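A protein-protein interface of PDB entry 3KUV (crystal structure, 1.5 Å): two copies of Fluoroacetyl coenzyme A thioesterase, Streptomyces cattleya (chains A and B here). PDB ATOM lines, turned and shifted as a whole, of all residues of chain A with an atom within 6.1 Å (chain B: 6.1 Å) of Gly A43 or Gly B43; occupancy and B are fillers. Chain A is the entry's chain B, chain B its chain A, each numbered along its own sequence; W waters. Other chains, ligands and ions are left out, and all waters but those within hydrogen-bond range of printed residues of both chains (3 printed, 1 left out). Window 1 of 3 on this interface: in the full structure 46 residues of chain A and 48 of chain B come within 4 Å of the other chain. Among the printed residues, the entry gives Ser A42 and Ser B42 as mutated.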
ATOM      1  N   LEU A  26      -8.222 -11.429 -33.039  1.00  0.00           N
ATOM      2  CA  LEU A  26      -7.560 -12.783 -32.992  1.00  0.00           C
ATOM      3  C   LEU A  26      -7.622 -13.527 -34.335  1.00  0.00           C
ATOM      4  O   LEU A  26      -6.650 -14.176 -34.726  1.00  0.00           O
ATOM      5  CB  LEU A  26      -8.198 -13.547 -31.818  1.00  0.00           C
ATOM      6  CG  LEU A  26      -7.491 -14.906 -31.519  1.00  0.00           C
ATOM      7  CD1 LEU A  26      -6.131 -14.661 -30.834  1.00  0.00           C
ATOM      8  CD2 LEU A  26      -8.417 -15.661 -30.585  1.00  0.00           C
ATOM      9  N   TYR A  27      -8.786 -13.457 -34.976  1.00  0.00           N
ATOM     10  CA  TYR A  27      -8.956 -14.009 -36.356  1.00  0.00           C
ATOM     11  C   TYR A  27      -9.641 -12.969 -37.227  1.00  0.00           C
ATOM     12  O   TYR A  27     -10.830 -13.028 -37.416  1.00  0.00           O
ATOM     13  CB  TYR A  27      -9.736 -15.344 -36.310  1.00  0.00           C
ATOM     14  CG  TYR A  27      -8.853 -16.503 -36.009  1.00  0.00           C
ATOM     15  CD1 TYR A  27      -8.209 -17.226 -36.994  1.00  0.00           C
ATOM     16  CD2 TYR A  27      -8.641 -16.885 -34.668  1.00  0.00           C
ATOM     17  CE1 TYR A  27      -7.382 -18.324 -36.734  1.00  0.00           C
ATOM     18  CE2 TYR A  27      -7.837 -18.005 -34.367  1.00  0.00           C
ATOM     19  CZ  TYR A  27      -7.145 -18.692 -35.367  1.00  0.00           C
ATOM     20  OH  TYR A  27      -6.350 -19.741 -35.137  1.00  0.00           O
ATOM     21  N   ALA A  41     -10.081 -11.264 -26.047  1.00  0.00           N
ATOM     22  CA  ALA A  41     -10.422 -12.643 -26.465  1.00  0.00           C
ATOM     23  C   ALA A  41      -9.850 -13.701 -25.562  1.00  0.00           C
ATOM     24  O   ALA A  41      -8.696 -13.533 -25.093  1.00  0.00           O
ATOM     25  CB  ALA A  41      -9.936 -12.947 -27.922  1.00  0.00           C
ATOM     26  N   SER A  42     -10.575 -14.829 -25.443  1.00  0.00           N
ATOM     27  CA  SER A  42     -10.075 -15.945 -24.678  1.00  0.00           C
ATOM     28  C   SER A  42      -8.666 -16.408 -25.162  1.00  0.00           C
ATOM     29  O   SER A  42      -7.829 -16.712 -24.336  1.00  0.00           O
ATOM     30  CB  SER A  42     -11.021 -17.117 -24.756  1.00  0.00           C
ATOM     31  OG  SER A  42     -12.204 -16.857 -24.044  1.00  0.00           O
ATOM     32  N   GLY A  43      -8.442 -16.438 -26.477  1.00  0.00           N
ATOM     33  CA  GLY A  43      -7.149 -16.932 -26.936  1.00  0.00           C
ATOM     34  C   GLY A  43      -6.050 -15.946 -26.534  1.00  0.00           C
ATOM     35  O   GLY A  43      -4.904 -16.351 -26.307  1.00  0.00           O
ATOM     36  N   PHE A  44      -6.356 -14.617 -26.523  1.00  0.00           N
ATOM     37  CA  PHE A  44      -5.379 -13.662 -26.022  1.00  0.00           C
ATOM     38  C   PHE A  44      -5.157 -13.825 -24.512  1.00  0.00           C
ATOM     39  O   PHE A  44      -4.023 -13.623 -24.030  1.00  0.00           O
ATOM     40  CB  PHE A  44      -5.753 -12.225 -26.379  1.00  0.00           C
ATOM     41  CG  PHE A  44      -5.542 -11.849 -27.848  1.00  0.00           C
ATOM     42  CD1 PHE A  44      -4.281 -11.987 -28.438  1.00  0.00           C
ATOM     43  CD2 PHE A  44      -6.588 -11.254 -28.576  1.00  0.00           C
ATOM     44  CE1 PHE A  44      -4.044 -11.586 -29.795  1.00  0.00           C
ATOM     45  CE2 PHE A  44      -6.416 -10.856 -29.889  1.00  0.00           C
ATOM     46  CZ  PHE A  44      -5.148 -10.991 -30.506  1.00  0.00           C
ATOM     47  N   MET A  45      -6.228 -14.100 -23.745  1.00  0.00           N
ATOM     48  CA  MET A  45      -6.002 -14.388 -22.327  1.00  0.00           C
ATOM     49  C   MET A  45      -5.135 -15.608 -22.113  1.00  0.00           C
ATOM     50  O   MET A  45      -4.203 -15.556 -21.247  1.00  0.00           O
ATOM     51  CB  MET A  45      -7.331 -14.550 -21.575  1.00  0.00           C
ATOM     52  CG  MET A  45      -7.170 -15.150 -20.123  1.00  0.00           C
ATOM     53  SD  MET A  45      -6.146 -13.924 -19.242  1.00  0.00           S
ATOM     54  CE  MET A  45      -7.450 -12.805 -18.811  1.00  0.00           C
ATOM     55  N   VAL A  46      -5.327 -16.663 -22.893  1.00  0.00           N
ATOM     56  CA  VAL A  46      -4.455 -17.840 -22.796  1.00  0.00           C
ATOM     57  C   VAL A  46      -3.009 -17.400 -23.047  1.00  0.00           C
ATOM     58  O   VAL A  46      -2.083 -17.750 -22.255  1.00  0.00           O
ATOM     59  CB  VAL A  46      -4.945 -18.916 -23.744  1.00  0.00           C
ATOM     60  CG1 VAL A  46      -3.888 -20.060 -23.851  1.00  0.00           C
ATOM     61  CG2 VAL A  46      -6.289 -19.531 -23.278  1.00  0.00           C
ATOM     62  N   GLY A  47      -2.776 -16.592 -24.098  1.00  0.00           N
ATOM     63  CA  GLY A  47      -1.384 -16.207 -24.406  1.00  0.00           C
ATOM     64  C   GLY A  47      -0.802 -15.347 -23.271  1.00  0.00           C
ATOM     65  O   GLY A  47       0.422 -15.362 -23.045  1.00  0.00           O
ATOM     66  N   LEU A  48      -1.621 -14.496 -22.646  1.00  0.00           N
ATOM     67  CA  LEU A  48      -1.118 -13.635 -21.571  1.00  0.00           C
ATOM     68  C   LEU A  48      -0.765 -14.458 -20.341  1.00  0.00           C
ATOM     69  O   LEU A  48       0.233 -14.119 -19.652  1.00  0.00           O
ATOM     70  CB  LEU A  48      -2.254 -12.631 -21.186  1.00  0.00           C
ATOM     71  CG  LEU A  48      -1.804 -11.513 -20.185  1.00  0.00           C
ATOM     72  CD1 LEU A  48      -0.795 -10.526 -20.864  1.00  0.00           C
ATOM     73  CD2 LEU A  48      -3.058 -10.746 -19.764  1.00  0.00           C
ATOM     74  N   GLU A  50       0.288 -17.579 -20.465  1.00  0.00           N
ATOM     75  CA  GLU A  50       1.562 -18.177 -20.850  1.00  0.00           C
ATOM     76  C   GLU A  50       2.684 -17.178 -20.620  1.00  0.00           C
ATOM     77  O   GLU A  50       3.736 -17.535 -20.100  1.00  0.00           O
ATOM     78  CB  GLU A  50       1.603 -18.623 -22.335  1.00  0.00           C
ATOM     79  CG  GLU A  50       0.630 -19.769 -22.607  1.00  0.00           C
ATOM     80  CD  GLU A  50       1.033 -20.451 -23.926  1.00  0.00           C
ATOM     81  OE1 GLU A  50       2.117 -21.091 -24.048  1.00  0.00           O
ATOM     82  OE2 GLU A  50       0.253 -20.370 -24.944  1.00  0.00           O
ATOM     83  N   LEU B  26       1.120 -13.527 -31.887  1.00  0.00           N
ATOM     84  CA  LEU B  26       0.040 -13.382 -30.840  1.00  0.00           C
ATOM     85  C   LEU B  26       0.241 -12.196 -29.936  1.00  0.00           C
ATOM     86  O   LEU B  26      -0.677 -11.394 -29.714  1.00  0.00           O
ATOM     87  CB  LEU B  26      -0.108 -14.726 -30.075  1.00  0.00           C
ATOM     88  CG  LEU B  26      -1.376 -14.729 -29.152  1.00  0.00           C
ATOM     89  CD1 LEU B  26      -2.673 -14.979 -29.976  1.00  0.00           C
ATOM     90  CD2 LEU B  26      -1.208 -15.898 -28.184  1.00  0.00           C
ATOM     91  N   TYR B  27       1.525 -12.030 -29.569  1.00  0.00           N
ATOM     92  CA  TYR B  27       1.944 -10.854 -28.748  1.00  0.00           C
ATOM     93  C   TYR B  27       3.253 -10.235 -29.301  1.00  0.00           C
ATOM     94  O   TYR B  27       4.377 -10.578 -28.819  1.00  0.00           O
ATOM     95  CB  TYR B  27       2.172 -11.239 -27.258  1.00  0.00           C
ATOM     96  CG  TYR B  27       0.851 -11.244 -26.508  1.00  0.00           C
ATOM     97  CD1 TYR B  27       0.321 -10.077 -26.024  1.00  0.00           C
ATOM     98  CD2 TYR B  27       0.120 -12.467 -26.366  1.00  0.00           C
ATOM     99  CE1 TYR B  27      -0.896 -10.076 -25.298  1.00  0.00           C
ATOM    100  CE2 TYR B  27      -1.121 -12.486 -25.684  1.00  0.00           C
ATOM    101  CZ  TYR B  27      -1.602 -11.321 -25.160  1.00  0.00           C
ATOM    102  OH  TYR B  27      -2.824 -11.312 -24.534  1.00  0.00           O
ATOM    103  N   ALA B  41       0.532 -20.722 -32.407  1.00  0.00           N
ATOM    104  CA  ALA B  41       0.483 -20.408 -30.951  1.00  0.00           C
ATOM    105  C   ALA B  41      -0.688 -21.100 -30.262  1.00  0.00           C
ATOM    106  O   ALA B  41      -1.783 -21.227 -30.856  1.00  0.00           O
ATOM    107  CB  ALA B  41       0.326 -18.915 -30.760  1.00  0.00           C
ATOM    108  N   SER B  42      -0.468 -21.542 -28.999  1.00  0.00           N
ATOM    109  CA  SER B  42      -1.615 -22.135 -28.266  1.00  0.00           C
ATOM    110  C   SER B  42      -2.820 -21.173 -28.302  1.00  0.00           C
ATOM    111  O   SER B  42      -3.985 -21.643 -28.410  1.00  0.00           O
ATOM    112  CB  SER B  42      -1.307 -22.558 -26.815  1.00  0.00           C
ATOM    113  OG  SER B  42      -0.151 -23.432 -26.760  1.00  0.00           O
ATOM    114  N   GLY B  43      -2.634 -19.865 -28.132  1.00  0.00           N
ATOM    115  CA  GLY B  43      -3.781 -18.971 -28.066  1.00  0.00           C
ATOM    116  C   GLY B  43      -4.535 -18.916 -29.403  1.00  0.00           C
ATOM    117  O   GLY B  43      -5.746 -18.729 -29.444  1.00  0.00           O
ATOM    118  N   PHE B  44      -3.797 -19.090 -30.504  1.00  0.00           N
ATOM    119  CA  PHE B  44      -4.494 -19.163 -31.803  1.00  0.00           C
ATOM    120  C   PHE B  44      -5.170 -20.552 -32.018  1.00  0.00           C
ATOM    121  O   PHE B  44      -6.268 -20.622 -32.589  1.00  0.00           O
ATOM    122  CB  PHE B  44      -3.499 -18.902 -32.956  1.00  0.00           C
ATOM    123  CG  PHE B  44      -3.119 -17.465 -33.143  1.00  0.00           C
ATOM    124  CD1 PHE B  44      -4.071 -16.467 -33.347  1.00  0.00           C
ATOM    125  CD2 PHE B  44      -1.727 -17.131 -33.251  1.00  0.00           C
ATOM    126  CE1 PHE B  44      -3.695 -15.088 -33.597  1.00  0.00           C
ATOM    127  CE2 PHE B  44      -1.369 -15.827 -33.451  1.00  0.00           C
ATOM    128  CZ  PHE B  44      -2.341 -14.770 -33.631  1.00  0.00           C
ATOM    129  N   MET B  45      -4.598 -21.642 -31.465  1.00  0.00           N
ATOM    130  CA  MET B  45      -5.287 -22.942 -31.496  1.00  0.00           C
ATOM    131  C   MET B  45      -6.623 -22.851 -30.688  1.00  0.00           C
ATOM    132  O   MET B  45      -7.683 -23.298 -31.157  1.00  0.00           O
ATOM    133  CB  MET B  45      -4.369 -24.045 -30.949  1.00  0.00           C
ATOM    134  CG  MET B  45      -5.157 -25.444 -30.971  1.00  0.00           C
ATOM    135  SD  MET B  45      -4.158 -26.806 -30.281  1.00  0.00           S
ATOM    136  CE  MET B  45      -4.401 -26.424 -28.511  1.00  0.00           C
ATOM    137  N   VAL B  46      -6.540 -22.220 -29.523  1.00  0.00           N
ATOM    138  CA  VAL B  46      -7.749 -21.981 -28.692  1.00  0.00           C
ATOM    139  C   VAL B  46      -8.791 -21.196 -29.497  1.00  0.00           C
ATOM    140  O   VAL B  46      -9.954 -21.626 -29.583  1.00  0.00           O
ATOM    141  CB  VAL B  46      -7.386 -21.375 -27.301  1.00  0.00           C
ATOM    142  CG1 VAL B  46      -8.643 -20.819 -26.604  1.00  0.00           C
ATOM    143  CG2 VAL B  46      -6.707 -22.406 -26.490  1.00  0.00           C
ATOM    144  N   GLY B  47      -8.350 -20.101 -30.183  1.00  0.00           N
ATOM    145  CA  GLY B  47      -9.309 -19.326 -30.959  1.00  0.00           C
ATOM    146  C   GLY B  47      -9.861 -20.123 -32.132  1.00  0.00           C
ATOM    147  O   GLY B  47     -11.068 -19.983 -32.380  1.00  0.00           O
ATOM    148  N   LEU B  48      -9.077 -21.000 -32.750  1.00  0.00           N
ATOM    149  CA  LEU B  48      -9.665 -21.824 -33.840  1.00  0.00           C
ATOM    150  C   LEU B  48     -10.693 -22.875 -33.317  1.00  0.00           C
ATOM    151  O   LEU B  48     -11.695 -23.149 -33.989  1.00  0.00           O
ATOM    152  CB  LEU B  48      -8.502 -22.528 -34.549  1.00  0.00           C
ATOM    153  CG  LEU B  48      -8.881 -23.347 -35.780  1.00  0.00           C
ATOM    154  CD1 LEU B  48      -9.355 -22.467 -36.878  1.00  0.00           C
ATOM    155  CD2 LEU B  48      -7.657 -24.183 -36.249  1.00  0.00           C
ATOM    156  N   GLU B  50     -12.523 -22.508 -30.623  1.00  0.00           N
ATOM    157  CA  GLU B  50     -13.720 -21.744 -30.232  1.00  0.00           C
ATOM    158  C   GLU B  50     -14.490 -21.300 -31.527  1.00  0.00           C
ATOM    159  O   GLU B  50     -15.729 -21.395 -31.563  1.00  0.00           O
ATOM    160  CB  GLU B  50     -13.292 -20.573 -29.295  1.00  0.00           C
ATOM    161  CG  GLU B  50     -12.684 -21.105 -27.996  1.00  0.00           C
ATOM    162  CD  GLU B  50     -12.267 -19.995 -27.020  1.00  0.00           C
ATOM    163  OE1 GLU B  50     -12.352 -18.809 -27.377  1.00  0.00           O
ATOM    164  OE2 GLU B  50     -11.873 -20.341 -25.874  1.00  0.00           O
ATOM    165  N   HIS B  76      -1.995 -29.320 -25.503  1.00  0.00           N
ATOM    166  CA  HIS B  76      -1.295 -28.966 -26.751  1.00  0.00           C
ATOM    167  C   HIS B  76      -0.108 -29.868 -26.829  1.00  0.00           C
ATOM    168  O   HIS B  76       0.859 -29.648 -26.085  1.00  0.00           O
ATOM    169  CB  HIS B  76      -0.981 -27.450 -26.740  1.00  0.00           C
ATOM    170  CG  HIS B  76      -0.677 -26.878 -28.115  1.00  0.00           C
ATOM    171  ND1 HIS B  76      -0.486 -25.540 -28.354  1.00  0.00           N
ATOM    172  CD2 HIS B  76      -0.679 -27.488 -29.316  1.00  0.00           C
ATOM    173  CE1 HIS B  76      -0.313 -25.357 -29.674  1.00  0.00           C
ATOM    174  NE2 HIS B  76      -0.371 -26.534 -30.260  1.00  0.00           N
HETATM  175  O   HOH W   1     -13.194 -19.782 -23.668  1.00  0.00           O
HETATM  176  O   HOH W   2      -0.412 -18.694 -26.742  1.00  0.00           O
HETATM  177  O   HOH W   3     -10.502 -16.968 -28.362  1.00  0.00           O
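Leu A26 touches Phe B44, and with the chains exchanged Phe A44 touches Leu B26. Leu A26 touches Gly B47, and with the chains exchanged Gly A47 touches Leu B26. Tyr A27 touches Gly B47, and with the chains exchanged Gly A47 touches Tyr B27. Ser A42 touches Glu B50, and with the chains exchanged Glu A50 touches Ser B42. 11 positions are printed for both chains.
The side-chain hydroxyl (OG) of Ser B42 sits at hydrogen-bond distance from a ring nitrogen (ND1) of His B76.
CD1 of Leu A26 touches CD1 of Leu B26 (3.6 Å). Phe B44 touches Leu A26 (CE1 to O, 3.3 Å). Leu A26 touches Gly B47. Glu B50 touches Ser A42. Gly A43 touches Gly B43 (O to CA, 3.3 Å). O of Leu B26 touches CE1 of Phe A44 (3.4 Å). Gly A47 touches Leu B26 (CA to CD2, 3.8 Å). Gly A47 touches Tyr B27 (C to CE2, 3.8 Å). Tyr B27 touches Leu A48 (OH to CB, 3.6 Å). Glu A50 touches Ser B42.
Of the 11 printed residues of chain A, 8 touch a printed residue of chain B. Of the 12 printed residues of chain B, 8 touch a printed residue of chain A. Among the printed residues, no Asp or Glu carboxylate lies within 4 Å of a Lys or Arg side-chain nitrogen of the other chain.
Water W2 lies within hydrogen-bond range of the side-chain carboxylate (OE2) of Glu A50 (2.5 Å) and the backbone NH (N) of Gly B43 (2.9 Å). Water W1 bridges the side-chain carboxylate (OE2) of Glu B50 (2.6 Å) and the side-chain hydroxyl (OG) of Ser A42 (3.1 Å). Water W3 lies within hydrogen-bond range of the side-chain carboxylate of Glu B50 (2.8 Å) and the backbone NH of Gly A43 (2.8 Å).
Printed residues of chain B within 4 Å of Gly A43: Gly B43. Printed residues of chain B within 4 Å of Ser A42: Glu B50 (3.4 Å). Printed residues of chain B within 4 Å of Gly A47: Leu B26 and Tyr B27. Of the printed residues of chain B, Phe A44 touches Leu B26 and Tyr B27. Printed residues of chain A within 4 Å of Phe B44: Leu A26 (3.3 Å) and Tyr A27 (2.7 Å). Printed residues of chain A within 4 Å of Leu B48: Tyr A27. His B76 touches none of the printed residues of chain A.
The side-chain hydroxyl (OH) of Tyr B27 is in hydrogen-bond range of the backbone carbonyl oxygen (O) of Phe A44 (2.7 Å). The backbone carbonyl oxygen (O) of Phe B44 is in hydrogen-bond range of the side-chain hydroxyl (OH) of Tyr A27 (2.7 Å).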
